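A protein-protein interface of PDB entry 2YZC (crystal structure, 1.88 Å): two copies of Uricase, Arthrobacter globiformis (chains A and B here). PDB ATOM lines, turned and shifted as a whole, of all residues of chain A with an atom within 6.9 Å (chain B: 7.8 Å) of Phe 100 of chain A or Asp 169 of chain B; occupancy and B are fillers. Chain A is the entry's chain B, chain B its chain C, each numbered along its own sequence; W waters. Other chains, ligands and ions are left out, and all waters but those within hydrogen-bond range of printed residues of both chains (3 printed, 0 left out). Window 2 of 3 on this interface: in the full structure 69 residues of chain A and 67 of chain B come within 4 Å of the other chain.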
ATOM      1  N   LEU A  48     -10.260 -27.028   5.884  1.00  0.00           N
ATOM      2  CA  LEU A  48     -10.258 -25.662   5.383  1.00  0.00           C
ATOM      3  C   LEU A  48      -8.863 -25.109   5.163  1.00  0.00           C
ATOM      4  O   LEU A  48      -7.907 -25.515   5.819  1.00  0.00           O
ATOM      5  CB  LEU A  48     -11.006 -24.764   6.369  1.00  0.00           C
ATOM      6  CG  LEU A  48     -12.350 -25.317   6.858  1.00  0.00           C
ATOM      7  CD1 LEU A  48     -13.006 -24.309   7.792  1.00  0.00           C
ATOM      8  CD2 LEU A  48     -13.254 -25.614   5.665  1.00  0.00           C
ATOM      9  N   HIS A  63     -10.022 -17.185  13.762  1.00  0.00           N
ATOM     10  CA  HIS A  63     -10.341 -17.687  12.428  1.00  0.00           C
ATOM     11  C   HIS A  63     -10.570 -19.193  12.407  1.00  0.00           C
ATOM     12  O   HIS A  63     -10.912 -19.756  11.371  1.00  0.00           O
ATOM     13  CB  HIS A  63      -9.213 -17.382  11.435  1.00  0.00           C
ATOM     14  CG  HIS A  63      -8.996 -15.924  11.175  1.00  0.00           C
ATOM     15  ND1 HIS A  63      -9.983 -14.977  11.352  1.00  0.00           N
ATOM     16  CD2 HIS A  63      -7.917 -15.256  10.699  1.00  0.00           C
ATOM     17  CE1 HIS A  63      -9.522 -13.792  10.996  1.00  0.00           C
ATOM     18  NE2 HIS A  63      -8.271 -13.933  10.595  1.00  0.00           N
ATOM     19  N   VAL A  65     -12.633 -22.086  12.657  1.00  0.00           N
ATOM     20  CA  VAL A  65     -13.976 -22.652  12.703  1.00  0.00           C
ATOM     21  C   VAL A  65     -13.766 -24.051  13.293  1.00  0.00           C
ATOM     22  O   VAL A  65     -13.105 -24.888  12.678  1.00  0.00           O
ATOM     23  CB  VAL A  65     -14.574 -22.766  11.277  1.00  0.00           C
ATOM     24  CG1 VAL A  65     -15.918 -23.470  11.321  1.00  0.00           C
ATOM     25  CG2 VAL A  65     -14.726 -21.379  10.666  1.00  0.00           C
ATOM     26  N   THR A  69     -17.755 -27.940  14.650  1.00  0.00           N
ATOM     27  CA  THR A  69     -18.744 -27.181  13.887  1.00  0.00           C
ATOM     28  C   THR A  69     -18.802 -27.696  12.453  1.00  0.00           C
ATOM     29  O   THR A  69     -19.874 -27.776  11.851  1.00  0.00           O
ATOM     30  CB  THR A  69     -18.402 -25.672  13.870  1.00  0.00           C
ATOM     31  OG1 THR A  69     -18.503 -25.148  15.200  1.00  0.00           O
ATOM     32  CG2 THR A  69     -19.349 -24.909  12.949  1.00  0.00           C
ATOM     33  N   THR A  73     -22.136 -29.303  10.605  1.00  0.00           N
ATOM     34  CA  THR A  73     -22.600 -28.814   9.318  1.00  0.00           C
ATOM     35  C   THR A  73     -22.868 -29.965   8.360  1.00  0.00           C
ATOM     36  O   THR A  73     -23.853 -29.946   7.626  1.00  0.00           O
ATOM     37  CB  THR A  73     -21.566 -27.853   8.695  1.00  0.00           C
ATOM     38  OG1 THR A  73     -21.288 -26.796   9.619  1.00  0.00           O
ATOM     39  CG2 THR A  73     -22.102 -27.256   7.402  1.00  0.00           C
ATOM     40  N   LYS A  94     -18.717 -24.864  -0.948  1.00  0.00           N
ATOM     41  CA  LYS A  94     -19.252 -23.539  -1.247  1.00  0.00           C
ATOM     42  C   LYS A  94     -19.580 -22.828   0.061  1.00  0.00           C
ATOM     43  O   LYS A  94     -19.225 -21.663   0.261  1.00  0.00           O
ATOM     44  CB  LYS A  94     -20.513 -23.662  -2.102  1.00  0.00           C
ATOM     45  CG  LYS A  94     -21.183 -22.334  -2.431  1.00  0.00           C
ATOM     46  CD  LYS A  94     -22.404 -22.545  -3.317  1.00  0.00           C
ATOM     47  CE  LYS A  94     -23.063 -21.223  -3.682  1.00  0.00           C
ATOM     48  NZ  LYS A  94     -22.143 -20.340  -4.452  1.00  0.00           N
ATOM     49  N   HIS A  95     -20.248 -23.546   0.956  1.00  0.00           N
ATOM     50  CA  HIS A  95     -20.628 -23.002   2.251  1.00  0.00           C
ATOM     51  C   HIS A  95     -19.460 -22.437   3.057  1.00  0.00           C
ATOM     52  O   HIS A  95     -19.524 -21.314   3.554  1.00  0.00           O
ATOM     53  CB  HIS A  95     -21.325 -24.078   3.092  1.00  0.00           C
ATOM     54  CG  HIS A  95     -21.505 -23.691   4.527  1.00  0.00           C
ATOM     55  ND1 HIS A  95     -22.438 -22.764   4.938  1.00  0.00           N
ATOM     56  CD2 HIS A  95     -20.835 -24.070   5.642  1.00  0.00           C
ATOM     57  CE1 HIS A  95     -22.335 -22.587   6.243  1.00  0.00           C
ATOM     58  NE2 HIS A  95     -21.368 -23.368   6.695  1.00  0.00           N
ATOM     59  N   PHE A  96     -18.397 -23.221   3.198  1.00  0.00           N
ATOM     60  CA  PHE A  96     -17.246 -22.785   3.982  1.00  0.00           C
ATOM     61  C   PHE A  96     -16.399 -21.684   3.347  1.00  0.00           C
ATOM     62  O   PHE A  96     -15.979 -20.751   4.035  1.00  0.00           O
ATOM     63  CB  PHE A  96     -16.363 -23.987   4.326  1.00  0.00           C
ATOM     64  CG  PHE A  96     -16.973 -24.906   5.351  1.00  0.00           C
ATOM     65  CD1 PHE A  96     -17.223 -24.454   6.646  1.00  0.00           C
ATOM     66  CD2 PHE A  96     -17.338 -26.203   5.013  1.00  0.00           C
ATOM     67  CE1 PHE A  96     -17.833 -25.283   7.590  1.00  0.00           C
ATOM     68  CE2 PHE A  96     -17.950 -27.040   5.951  1.00  0.00           C
ATOM     69  CZ  PHE A  96     -18.196 -26.577   7.240  1.00  0.00           C
ATOM     70  N   THR A  97     -16.142 -21.782   2.049  1.00  0.00           N
ATOM     71  CA  THR A  97     -15.326 -20.768   1.389  1.00  0.00           C
ATOM     72  C   THR A  97     -16.028 -19.413   1.328  1.00  0.00           C
ATOM     73  O   THR A  97     -15.398 -18.371   1.508  1.00  0.00           O
ATOM     74  CB  THR A  97     -14.927 -21.204  -0.037  1.00  0.00           C
ATOM     75  OG1 THR A  97     -16.102 -21.477  -0.808  1.00  0.00           O
ATOM     76  CG2 THR A  97     -14.058 -22.460   0.018  1.00  0.00           C
ATOM     77  N   GLU A  98     -17.333 -19.429   1.090  1.00  0.00           N
ATOM     78  CA  GLU A  98     -18.104 -18.196   1.004  1.00  0.00           C
ATOM     79  C   GLU A  98     -18.616 -17.691   2.349  1.00  0.00           C
ATOM     80  O   GLU A  98     -18.787 -16.485   2.544  1.00  0.00           O
ATOM     81  CB  GLU A  98     -19.281 -18.391   0.048  1.00  0.00           C
ATOM     82  CG  GLU A  98     -18.888 -18.338  -1.418  1.00  0.00           C
ATOM     83  CD  GLU A  98     -20.029 -18.714  -2.339  1.00  0.00           C
ATOM     84  OE1 GLU A  98     -21.196 -18.435  -1.986  1.00  0.00           O
ATOM     85  OE2 GLU A  98     -19.759 -19.279  -3.421  1.00  0.00           O
ATOM     86  N   GLY A  99     -18.851 -18.610   3.279  1.00  0.00           N
ATOM     87  CA  GLY A  99     -19.363 -18.222   4.580  1.00  0.00           C
ATOM     88  C   GLY A  99     -18.359 -17.568   5.507  1.00  0.00           C
ATOM     89  O   GLY A  99     -18.737 -16.984   6.519  1.00  0.00           O
ATOM     90  N   PHE A 100     -17.080 -17.663   5.166  1.00  0.00           N
ATOM     91  CA  PHE A 100     -16.027 -17.080   5.986  1.00  0.00           C
ATOM     92  C   PHE A 100     -15.007 -16.391   5.086  1.00  0.00           C
ATOM     93  O   PHE A 100     -14.456 -17.003   4.173  1.00  0.00           O
ATOM     94  CB  PHE A 100     -15.357 -18.178   6.816  1.00  0.00           C
ATOM     95  CG  PHE A 100     -16.303 -18.890   7.741  1.00  0.00           C
ATOM     96  CD1 PHE A 100     -16.639 -18.340   8.975  1.00  0.00           C
ATOM     97  CD2 PHE A 100     -16.891 -20.094   7.363  1.00  0.00           C
ATOM     98  CE1 PHE A 100     -17.547 -18.976   9.818  1.00  0.00           C
ATOM     99  CE2 PHE A 100     -17.802 -20.737   8.201  1.00  0.00           C
ATOM    100  CZ  PHE A 100     -18.130 -20.176   9.432  1.00  0.00           C
ATOM    101  N   ASP A 101     -14.763 -15.112   5.352  1.00  0.00           N
ATOM    102  CA  ASP A 101     -13.833 -14.320   4.555  1.00  0.00           C
ATOM    103  C   ASP A 101     -12.391 -14.803   4.567  1.00  0.00           C
ATOM    104  O   ASP A 101     -11.719 -14.768   3.539  1.00  0.00           O
ATOM    105  CB  ASP A 101     -13.874 -12.857   5.001  1.00  0.00           C
ATOM    106  CG  ASP A 101     -15.231 -12.220   4.770  1.00  0.00           C
ATOM    107  OD1 ASP A 101     -15.773 -12.381   3.657  1.00  0.00           O
ATOM    108  OD2 ASP A 101     -15.751 -11.556   5.694  1.00  0.00           O
ATOM    109  N   TRP A 102     -11.911 -15.252   5.722  1.00  0.00           N
ATOM    110  CA  TRP A 102     -10.534 -15.715   5.826  1.00  0.00           C
ATOM    111  C   TRP A 102     -10.312 -17.119   5.263  1.00  0.00           C
ATOM    112  O   TRP A 102      -9.170 -17.554   5.121  1.00  0.00           O
ATOM    113  CB  TRP A 102     -10.068 -15.649   7.282  1.00  0.00           C
ATOM    114  CG  TRP A 102     -10.868 -16.497   8.202  1.00  0.00           C
ATOM    115  CD1 TRP A 102     -10.748 -17.842   8.391  1.00  0.00           C
ATOM    116  CD2 TRP A 102     -11.939 -16.065   9.046  1.00  0.00           C
ATOM    117  NE1 TRP A 102     -11.680 -18.277   9.302  1.00  0.00           N
ATOM    118  CE2 TRP A 102     -12.425 -17.206   9.720  1.00  0.00           C
ATOM    119  CE3 TRP A 102     -12.535 -14.823   9.298  1.00  0.00           C
ATOM    120  CZ2 TRP A 102     -13.481 -17.144  10.634  1.00  0.00           C
ATOM    121  CZ3 TRP A 102     -13.586 -14.760  10.208  1.00  0.00           C
ATOM    122  CH2 TRP A 102     -14.048 -15.915  10.864  1.00  0.00           C
ATOM    123  N   VAL A 103     -11.398 -17.828   4.960  1.00  0.00           N
ATOM    124  CA  VAL A 103     -11.292 -19.162   4.376  1.00  0.00           C
ATOM    125  C   VAL A 103     -11.359 -18.982   2.862  1.00  0.00           C
ATOM    126  O   VAL A 103     -12.391 -18.585   2.321  1.00  0.00           O
ATOM    127  CB  VAL A 103     -12.442 -20.085   4.834  1.00  0.00           C
ATOM    128  CG1 VAL A 103     -12.349 -21.432   4.116  1.00  0.00           C
ATOM    129  CG2 VAL A 103     -12.372 -20.284   6.343  1.00  0.00           C
ATOM    130  N   THR A 104     -10.253 -19.271   2.185  1.00  0.00           N
ATOM    131  CA  THR A 104     -10.174 -19.103   0.735  1.00  0.00           C
ATOM    132  C   THR A 104     -10.277 -20.397  -0.061  1.00  0.00           C
ATOM    133  O   THR A 104     -10.304 -20.377  -1.293  1.00  0.00           O
ATOM    134  CB  THR A 104      -8.862 -18.402   0.343  1.00  0.00           C
ATOM    135  OG1 THR A 104      -7.750 -19.191   0.784  1.00  0.00           O
ATOM    136  CG2 THR A 104      -8.781 -17.028   0.989  1.00  0.00           C
ATOM    137  N   PHE B 166     -12.970 -19.305  19.449  1.00  0.00           N
ATOM    138  CA  PHE B 166     -13.302 -19.658  18.074  1.00  0.00           C
ATOM    139  C   PHE B 166     -14.646 -19.062  17.680  1.00  0.00           C
ATOM    140  O   PHE B 166     -15.509 -18.838  18.531  1.00  0.00           O
ATOM    141  CB  PHE B 166     -13.331 -21.178  17.886  1.00  0.00           C
ATOM    142  CG  PHE B 166     -14.100 -21.919  18.948  1.00  0.00           C
ATOM    143  CD1 PHE B 166     -13.470 -22.333  20.117  1.00  0.00           C
ATOM    144  CD2 PHE B 166     -15.441 -22.232  18.761  1.00  0.00           C
ATOM    145  CE1 PHE B 166     -14.166 -23.055  21.084  1.00  0.00           C
ATOM    146  CE2 PHE B 166     -16.149 -22.954  19.722  1.00  0.00           C
ATOM    147  CZ  PHE B 166     -15.511 -23.366  20.884  1.00  0.00           C
ATOM    148  N   PRO B 167     -14.841 -18.789  16.380  1.00  0.00           N
ATOM    149  CA  PRO B 167     -16.108 -18.212  15.919  1.00  0.00           C
ATOM    150  C   PRO B 167     -17.296 -19.133  16.185  1.00  0.00           C
ATOM    151  O   PRO B 167     -17.156 -20.355  16.199  1.00  0.00           O
ATOM    152  CB  PRO B 167     -15.857 -17.977  14.430  1.00  0.00           C
ATOM    153  CG  PRO B 167     -14.876 -19.058  14.075  1.00  0.00           C
ATOM    154  CD  PRO B 167     -13.929 -19.034  15.249  1.00  0.00           C
ATOM    155  N   ARG B 168     -18.464 -18.542  16.409  1.00  0.00           N
ATOM    156  CA  ARG B 168     -19.661 -19.328  16.673  1.00  0.00           C
ATOM    157  C   ARG B 168     -20.770 -18.997  15.686  1.00  0.00           C
ATOM    158  O   ARG B 168     -21.305 -17.887  15.690  1.00  0.00           O
ATOM    159  CB  ARG B 168     -20.166 -19.074  18.098  1.00  0.00           C
ATOM    160  CG  ARG B 168     -19.114 -19.242  19.184  1.00  0.00           C
ATOM    161  CD  ARG B 168     -19.731 -19.105  20.570  1.00  0.00           C
ATOM    162  NE  ARG B 168     -20.539 -20.269  20.931  1.00  0.00           N
ATOM    163  CZ  ARG B 168     -20.037 -21.456  21.258  1.00  0.00           C
ATOM    164  NH1 ARG B 168     -18.724 -21.642  21.276  1.00  0.00           N
ATOM    165  NH2 ARG B 168     -20.847 -22.461  21.566  1.00  0.00           N
ATOM    166  N   ASP B 169     -21.112 -19.955  14.832  1.00  0.00           N
ATOM    167  CA  ASP B 169     -22.182 -19.741  13.868  1.00  0.00           C
ATOM    168  C   ASP B 169     -23.367 -20.603  14.286  1.00  0.00           C
ATOM    169  O   ASP B 169     -23.325 -21.244  15.336  1.00  0.00           O
ATOM    170  CB  ASP B 169     -21.717 -20.086  12.446  1.00  0.00           C
ATOM    171  CG  ASP B 169     -21.399 -21.560  12.263  1.00  0.00           C
ATOM    172  OD1 ASP B 169     -21.490 -22.328  13.243  1.00  0.00           O
ATOM    173  OD2 ASP B 169     -21.055 -21.947  11.124  1.00  0.00           O
ATOM    174  N   LYS B 170     -24.421 -20.622  13.477  1.00  0.00           N
ATOM    175  CA  LYS B 170     -25.602 -21.406  13.819  1.00  0.00           C
ATOM    176  C   LYS B 170     -25.333 -22.896  14.011  1.00  0.00           C
ATOM    177  O   LYS B 170     -26.135 -23.587  14.635  1.00  0.00           O
ATOM    178  CB  LYS B 170     -26.696 -21.236  12.757  1.00  0.00           C
ATOM    179  CG  LYS B 170     -26.372 -21.849  11.410  1.00  0.00           C
ATOM    180  CD  LYS B 170     -27.637 -22.359  10.721  1.00  0.00           C
ATOM    181  CE  LYS B 170     -28.665 -21.254  10.517  1.00  0.00           C
ATOM    182  NZ  LYS B 170     -29.922 -21.771   9.900  1.00  0.00           N
ATOM    183  N   TYR B 171     -24.212 -23.387  13.487  1.00  0.00           N
ATOM    184  CA  TYR B 171     -23.884 -24.806  13.602  1.00  0.00           C
ATOM    185  C   TYR B 171     -22.866 -25.108  14.694  1.00  0.00           C
ATOM    186  O   TYR B 171     -22.378 -26.236  14.798  1.00  0.00           O
ATOM    187  CB  TYR B 171     -23.350 -25.335  12.266  1.00  0.00           C
ATOM    188  CG  TYR B 171     -24.287 -25.121  11.100  1.00  0.00           C
ATOM    189  CD1 TYR B 171     -25.504 -25.797  11.022  1.00  0.00           C
ATOM    190  CD2 TYR B 171     -23.966 -24.220  10.085  1.00  0.00           C
ATOM    191  CE1 TYR B 171     -26.382 -25.579   9.961  1.00  0.00           C
ATOM    192  CE2 TYR B 171     -24.831 -23.995   9.021  1.00  0.00           C
ATOM    193  CZ  TYR B 171     -26.035 -24.674   8.964  1.00  0.00           C
ATOM    194  OH  TYR B 171     -26.896 -24.434   7.919  1.00  0.00           O
ATOM    195  N   THR B 172     -22.543 -24.108  15.502  1.00  0.00           N
ATOM    196  CA  THR B 172     -21.571 -24.283  16.577  1.00  0.00           C
ATOM    197  C   THR B 172     -22.242 -24.594  17.912  1.00  0.00           C
ATOM    198  O   THR B 172     -23.074 -23.823  18.394  1.00  0.00           O
ATOM    199  CB  THR B 172     -20.697 -23.022  16.740  1.00  0.00           C
ATOM    200  OG1 THR B 172     -20.068 -22.714  15.488  1.00  0.00           O
ATOM    201  CG2 THR B 172     -19.622 -23.247  17.790  1.00  0.00           C
ATOM    202  N   THR B 173     -21.876 -25.728  18.503  1.00  0.00           N
ATOM    203  CA  THR B 173     -22.433 -26.138  19.788  1.00  0.00           C
ATOM    204  C   THR B 173     -21.316 -26.408  20.789  1.00  0.00           C
ATOM    205  O   THR B 173     -21.566 -26.564  21.987  1.00  0.00           O
ATOM    206  CB  THR B 173     -23.277 -27.424  19.651  1.00  0.00           C
ATOM    207  OG1 THR B 173     -22.444 -28.500  19.204  1.00  0.00           O
ATOM    208  CG2 THR B 173     -24.402 -27.217  18.653  1.00  0.00           C
HETATM  209  O   HOH W   1     -16.585 -22.678  15.060  1.00  0.00           O
HETATM  210  O   HOH W   2     -19.571 -26.928  17.364  1.00  0.00           O
HETATM  211  O   HOH W   3     -20.387 -24.068   9.455  1.00  0.00           O
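No position is printed for both chains. Of the 7 pairs that touch across the chains among the printed residues, none has its exchanged pair printed and touching as well.
Water W1 bridges the backbone carbonyl oxygen (O) of Pro 167 of chain B (2.6 Å) and the side-chain hydroxyl (OG1) of Thr 69 of chain A (3.1 Å). Water W3 lies within hydrogen-bond range of OD2 of Asp 169 of chain B (2.8 Å), OG1 of Thr 73 of chain A (2.9 Å) and NE2 of His 95 of chain A (3.0 Å). Water W2 lies within hydrogen-bond range of N of Thr 173 of chain B (2.8 Å) and OG1 of Thr 69 of chain A (3.0 Å).
Of the 16 printed residues of chain A, 5 touch a printed residue of chain B. Hydrophobic or aromatic side chains of chain A within 4 Å of the printed part of chain B: His 95 and Phe 100. Among the printed residues, 7 pairs touch across the chains.
The side-chain carboxylate (OD1) of Asp 169 of chain B lies within hydrogen-bond range of the backbone NH (N) of Tyr 171 of chain B (2.9 Å). The side-chain hydroxyl (OG1) of Thr 172 of chain B lies within hydrogen-bond range of the side-chain carboxylate (OD1) of Asp 169 of chain B. The side-chain hydroxyl of Thr 73 of chain A sits at hydrogen-bond distance from the backbone carbonyl oxygen of Thr 69 of chain A (2.8 Å).
Of chain A, only Thr 69 (3.4 Å) and Phe 100 (3.8 Å) come within 4 Å of Asp 169 of chain B. No residue of chain B comes within 4 Å of Gly 99 of chain A. Of the printed residues of chain B, Val 65 of chain A touches Pro 167. Printed residues of chain B within 4 Å of Thr 73 of chain A: Tyr 171 (3.7 Å). Of the printed residues of chain A, Thr 172 of chain B touches Thr 69 (2.9 Å). Phe 96 of chain A touches none of the printed residues of chain B. The nearest residue of chain A that does not touch Asp 169 of chain B is His 95 of chain A (4.7 Å). The nearest printed residue of chain A that does not touch Thr 172 of chain B is Val 65 of chain A (5.9 Å).
The side-chain hydroxyl of Thr 69 of chain A is in hydrogen-bond range of the side-chain hydroxyl of Thr 172 of chain B (2.9 Å).
Val 65 of chain A touches Pro 167 of chain B. CG2 of Thr 69 of chain A touches OD1 of Asp 169 of chain B, at 3.4 Å. O of Tyr 171 of chain B touches CG2 of Thr 69 of chain A (3.8 Å). CB of Tyr 171 of chain B touches OG1 of Thr 73 of chain A, at 3.7 Å. CE1 of His 95 of chain A touches CE2 of Tyr 171 of chain B (3.99 Å). OD2 of Asp 169 of chain B touches CZ of Phe 100 of chain A, 3.8 Å away.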
